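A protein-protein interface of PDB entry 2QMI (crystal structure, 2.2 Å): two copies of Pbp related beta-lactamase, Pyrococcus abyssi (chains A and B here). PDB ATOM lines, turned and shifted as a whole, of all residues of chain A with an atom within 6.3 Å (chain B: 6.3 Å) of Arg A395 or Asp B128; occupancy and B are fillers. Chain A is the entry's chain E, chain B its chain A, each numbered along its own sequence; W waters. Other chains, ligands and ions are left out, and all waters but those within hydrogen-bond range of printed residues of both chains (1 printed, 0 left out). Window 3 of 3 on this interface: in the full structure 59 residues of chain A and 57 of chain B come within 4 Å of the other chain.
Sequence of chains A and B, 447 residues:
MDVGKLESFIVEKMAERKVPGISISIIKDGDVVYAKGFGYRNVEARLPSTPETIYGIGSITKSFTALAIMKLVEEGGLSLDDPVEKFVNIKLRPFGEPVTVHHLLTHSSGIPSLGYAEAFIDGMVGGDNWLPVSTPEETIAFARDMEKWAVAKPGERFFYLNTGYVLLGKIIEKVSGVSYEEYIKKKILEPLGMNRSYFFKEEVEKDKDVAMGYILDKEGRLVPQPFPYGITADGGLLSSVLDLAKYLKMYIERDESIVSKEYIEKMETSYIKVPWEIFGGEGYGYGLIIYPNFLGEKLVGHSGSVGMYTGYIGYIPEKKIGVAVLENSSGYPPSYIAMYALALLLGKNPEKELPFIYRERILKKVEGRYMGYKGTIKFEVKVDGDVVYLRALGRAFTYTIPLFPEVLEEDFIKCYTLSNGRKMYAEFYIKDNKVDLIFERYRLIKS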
ATOM      1  N   LYS A 378     -15.293 -21.283 -15.408  1.00  0.00           N
ATOM      2  CA  LYS A 378     -13.870 -21.284 -15.088  1.00  0.00           C
ATOM      3  C   LYS A 378     -13.203 -22.535 -15.630  1.00  0.00           C
ATOM      4  O   LYS A 378     -13.798 -23.612 -15.637  1.00  0.00           O
ATOM      5  CB  LYS A 378     -13.646 -21.249 -13.568  1.00  0.00           C
ATOM      6  CG  LYS A 378     -14.263 -20.068 -12.821  1.00  0.00           C
ATOM      7  CD  LYS A 378     -15.752 -20.266 -12.542  1.00  0.00           C
ATOM      8  CE  LYS A 378     -16.285 -19.102 -11.697  1.00  0.00           C
ATOM      9  NZ  LYS A 378     -17.772 -19.093 -11.528  1.00  0.00           N
ATOM     10  N   LEU A 393     -13.109 -26.063 -14.282  1.00  0.00           N
ATOM     11  CA  LEU A 393     -13.101 -26.017 -12.827  1.00  0.00           C
ATOM     12  C   LEU A 393     -14.503 -26.314 -12.265  1.00  0.00           C
ATOM     13  O   LEU A 393     -15.470 -26.439 -13.023  1.00  0.00           O
ATOM     14  CB  LEU A 393     -12.608 -24.644 -12.362  1.00  0.00           C
ATOM     15  CG  LEU A 393     -11.201 -24.251 -12.830  1.00  0.00           C
ATOM     16  CD1 LEU A 393     -10.816 -22.911 -12.230  1.00  0.00           C
ATOM     17  CD2 LEU A 393     -10.193 -25.315 -12.408  1.00  0.00           C
ATOM     18  N   GLY A 394     -14.612 -26.416 -10.942  1.00  0.00           N
ATOM     19  CA  GLY A 394     -15.895 -26.715 -10.320  1.00  0.00           C
ATOM     20  C   GLY A 394     -15.842 -28.093  -9.672  1.00  0.00           C
ATOM     21  O   GLY A 394     -15.931 -29.109 -10.361  1.00  0.00           O
ATOM     22  N   ARG A 395     -15.708 -28.127  -8.347  1.00  0.00           N
ATOM     23  CA  ARG A 395     -15.598 -29.378  -7.582  1.00  0.00           C
ATOM     24  C   ARG A 395     -16.502 -30.565  -7.944  1.00  0.00           C
ATOM     25  O   ARG A 395     -16.016 -31.696  -8.086  1.00  0.00           O
ATOM     26  CB  ARG A 395     -15.756 -29.083  -6.091  1.00  0.00           C
ATOM     27  CG  ARG A 395     -14.739 -28.094  -5.555  1.00  0.00           C
ATOM     28  CD  ARG A 395     -15.081 -27.730  -4.121  1.00  0.00           C
ATOM     29  NE  ARG A 395     -16.462 -27.263  -4.021  1.00  0.00           N
ATOM     30  CZ  ARG A 395     -17.048 -26.883  -2.891  1.00  0.00           C
ATOM     31  NH1 ARG A 395     -16.377 -26.917  -1.746  1.00  0.00           N
ATOM     32  NH2 ARG A 395     -18.308 -26.459  -2.912  1.00  0.00           N
ATOM     33  N   ALA A 396     -17.807 -30.333  -8.059  1.00  0.00           N
ATOM     34  CA  ALA A 396     -18.722 -31.424  -8.394  1.00  0.00           C
ATOM     35  C   ALA A 396     -18.265 -32.082  -9.689  1.00  0.00           C
ATOM     36  O   ALA A 396     -18.245 -33.315  -9.808  1.00  0.00           O
ATOM     37  CB  ALA A 396     -20.150 -30.898  -8.546  1.00  0.00           C
ATOM     38  N   PHE A 397     -17.889 -31.242 -10.651  1.00  0.00           N
ATOM     39  CA  PHE A 397     -17.427 -31.691 -11.962  1.00  0.00           C
ATOM     40  C   PHE A 397     -15.953 -31.305 -12.116  1.00  0.00           C
ATOM     41  O   PHE A 397     -15.247 -31.161 -11.116  1.00  0.00           O
ATOM     42  CB  PHE A 397     -18.259 -30.999 -13.044  1.00  0.00           C
ATOM     43  CG  PHE A 397     -19.738 -31.059 -12.797  1.00  0.00           C
ATOM     44  CD1 PHE A 397     -20.468 -32.204 -13.132  1.00  0.00           C
ATOM     45  CD2 PHE A 397     -20.393 -29.995 -12.180  1.00  0.00           C
ATOM     46  CE1 PHE A 397     -21.831 -32.291 -12.851  1.00  0.00           C
ATOM     47  CE2 PHE A 397     -21.757 -30.069 -11.895  1.00  0.00           C
ATOM     48  CZ  PHE A 397     -22.479 -31.224 -12.229  1.00  0.00           C
ATOM     49  N   THR A 398     -15.504 -31.152 -13.362  1.00  0.00           N
ATOM     50  CA  THR A 398     -14.127 -30.740 -13.694  1.00  0.00           C
ATOM     51  C   THR A 398     -13.430 -31.637 -14.728  1.00  0.00           C
ATOM     52  O   THR A 398     -12.272 -32.037 -14.542  1.00  0.00           O
ATOM     53  CB  THR A 398     -13.209 -30.614 -12.419  1.00  0.00           C
ATOM     54  OG1 THR A 398     -12.037 -29.853 -12.746  1.00  0.00           O
ATOM     55  CG2 THR A 398     -12.777 -32.000 -11.896  1.00  0.00           C
ATOM     56  N   ASP B 122     -25.528 -25.221 -13.762  1.00  0.00           N
ATOM     57  CA  ASP B 122     -24.568 -25.779 -12.814  1.00  0.00           C
ATOM     58  C   ASP B 122     -24.926 -25.431 -11.366  1.00  0.00           C
ATOM     59  O   ASP B 122     -24.957 -26.302 -10.501  1.00  0.00           O
ATOM     60  CB  ASP B 122     -23.157 -25.275 -13.125  1.00  0.00           C
ATOM     61  CG  ASP B 122     -22.088 -25.975 -12.292  1.00  0.00           C
ATOM     62  OD1 ASP B 122     -21.893 -27.192 -12.482  1.00  0.00           O
ATOM     63  OD2 ASP B 122     -21.450 -25.312 -11.443  1.00  0.00           O
ATOM     64  N   GLY B 123     -25.192 -24.156 -11.105  1.00  0.00           N
ATOM     65  CA  GLY B 123     -25.533 -23.748  -9.753  1.00  0.00           C
ATOM     66  C   GLY B 123     -26.865 -24.307  -9.292  1.00  0.00           C
ATOM     67  O   GLY B 123     -27.057 -24.599  -8.116  1.00  0.00           O
ATOM     68  N   GLY B 126     -26.491 -27.937  -7.468  1.00  0.00           N
ATOM     69  CA  GLY B 126     -25.463 -28.154  -6.464  1.00  0.00           C
ATOM     70  C   GLY B 126     -24.052 -27.796  -6.898  1.00  0.00           C
ATOM     71  O   GLY B 126     -23.113 -27.903  -6.103  1.00  0.00           O
ATOM     72  N   GLY B 127     -23.888 -27.377  -8.150  1.00  0.00           N
ATOM     73  CA  GLY B 127     -22.562 -27.011  -8.638  1.00  0.00           C
ATOM     74  C   GLY B 127     -21.929 -25.838  -7.899  1.00  0.00           C
ATOM     75  O   GLY B 127     -22.557 -25.223  -7.033  1.00  0.00           O
ATOM     76  N   ASP B 128     -20.687 -25.508  -8.245  1.00  0.00           N
ATOM     77  CA  ASP B 128     -19.991 -24.410  -7.583  1.00  0.00           C
ATOM     78  C   ASP B 128     -20.235 -22.986  -8.107  1.00  0.00           C
ATOM     79  O   ASP B 128     -20.167 -22.033  -7.322  1.00  0.00           O
ATOM     80  CB  ASP B 128     -18.481 -24.684  -7.538  1.00  0.00           C
ATOM     81  CG  ASP B 128     -18.109 -25.707  -6.478  1.00  0.00           C
ATOM     82  OD1 ASP B 128     -18.692 -25.644  -5.368  1.00  0.00           O
ATOM     83  OD2 ASP B 128     -17.234 -26.563  -6.740  1.00  0.00           O
ATOM     84  N   ASN B 129     -20.509 -22.803  -9.398  1.00  0.00           N
ATOM     85  CA  ASN B 129     -20.751 -21.439  -9.855  1.00  0.00           C
ATOM     86  C   ASN B 129     -22.197 -21.020  -9.620  1.00  0.00           C
ATOM     87  O   ASN B 129     -22.975 -21.760  -9.005  1.00  0.00           O
ATOM     88  CB  ASN B 129     -20.348 -21.238 -11.326  1.00  0.00           C
ATOM     89  CG  ASN B 129     -20.756 -22.380 -12.200  1.00  0.00           C
ATOM     90  OD1 ASN B 129     -21.888 -22.865 -12.110  1.00  0.00           O
ATOM     91  ND2 ASN B 129     -19.845 -22.822 -13.066  1.00  0.00           N
ATOM     92  N   TRP B 130     -22.563 -19.837 -10.106  1.00  0.00           N
ATOM     93  CA  TRP B 130     -23.908 -19.328  -9.869  1.00  0.00           C
ATOM     94  C   TRP B 130     -24.269 -18.156 -10.786  1.00  0.00           C
ATOM     95  O   TRP B 130     -23.448 -17.281 -11.038  1.00  0.00           O
ATOM     96  CB  TRP B 130     -23.996 -18.902  -8.395  1.00  0.00           C
ATOM     97  CG  TRP B 130     -25.373 -18.595  -7.879  1.00  0.00           C
ATOM     98  CD1 TRP B 130     -25.876 -17.364  -7.567  1.00  0.00           C
ATOM     99  CD2 TRP B 130     -26.415 -19.540  -7.588  1.00  0.00           C
ATOM    100  NE1 TRP B 130     -27.162 -17.482  -7.099  1.00  0.00           N
ATOM    101  CE2 TRP B 130     -27.520 -18.804  -7.101  1.00  0.00           C
ATOM    102  CE3 TRP B 130     -26.522 -20.933  -7.691  1.00  0.00           C
ATOM    103  CZ2 TRP B 130     -28.721 -19.418  -6.715  1.00  0.00           C
ATOM    104  CZ3 TRP B 130     -27.719 -21.543  -7.308  1.00  0.00           C
ATOM    105  CH2 TRP B 130     -28.801 -20.781  -6.824  1.00  0.00           C
ATOM    106  N   LYS B 218     -20.059 -38.009  -8.721  1.00  0.00           N
ATOM    107  CA  LYS B 218     -18.714 -38.553  -8.896  1.00  0.00           C
ATOM    108  C   LYS B 218     -18.564 -39.947  -8.306  1.00  0.00           C
ATOM    109  O   LYS B 218     -17.698 -40.720  -8.727  1.00  0.00           O
ATOM    110  CB  LYS B 218     -17.664 -37.594  -8.303  1.00  0.00           C
ATOM    111  CG  LYS B 218     -18.166 -36.728  -7.156  1.00  0.00           C
ATOM    112  CD  LYS B 218     -17.237 -35.528  -6.928  1.00  0.00           C
ATOM    113  CE  LYS B 218     -17.822 -34.526  -5.908  1.00  0.00           C
ATOM    114  NZ  LYS B 218     -18.142 -35.183  -4.595  1.00  0.00           N
HETATM  115  O   HOH W   1     -18.946 -27.499 -10.203  1.00  0.00           O
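OD1 of Asp B128 lies within salt-bridge range of NH2 of Arg A395 (2.6 Å).
Among the printed residues, merely in contact across the chains: Phe A397 with Asp B122 (2.9 Å), Lys A378 with Asn B129 (3.4 Å), Gly A394 with Asp B128 (3.6 Å) and Ala A396 with Lys B218 (3.8 Å).
The backbone carbonyl oxygen (O) of Asp B122 sits at hydrogen-bond distance from the backbone NH (N) of Gly B127, 2.8 Å away.
The backbone NH of Leu A393 sits at hydrogen-bond distance from the backbone carbonyl oxygen of Lys A378, at 2.9 Å.
N of Asp B128 sits at hydrogen-bond distance from OD2 of Asp B122 (3.3 Å).
The side-chain carboxylate (OD2) of Asp B122 lies close to the side-chain amide oxygen (OD1) of Asn B129 (2.6 Å).
No position is printed for both chains.
Water W1 lies within hydrogen-bond range of N of Asp B128 (3.3 Å) and O of Gly A394 (3.4 Å).
Printed residues of chain B within 4 Å of Arg A395: Asp B128.
Of chain A, only Gly A394 (3.6 Å) and Arg A395 (2.6 Å) come within 4 Å of Asp B128.
Of the printed residues of chain A, Asn B129 touches Lys A378 (3.4 Å).
Printed residues of chain A within 4 Å of Asp B122: Phe A397.
Thr A398 touches none of the printed residues of chain B.
Gly B127 touches none of the printed residues of chain A.
The nearest printed residue of chain B that does not touch Arg A395 is Lys B218 (4.002 Å).
The nearest printed residue of chain B that does not touch Lys A378 is Trp B130 (5.1 Å).
Of the 8 printed residues of chain B, 4 touch a printed residue of chain A.
Of the 7 printed residues of chain A, 5 touch a printed residue of chain B.
Among the printed residues, Asp or Glu carboxylates within 4 Å of a Lys or Arg side-chain nitrogen of the other chain: Arg A395 with Asp B128 (2.6 Å).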
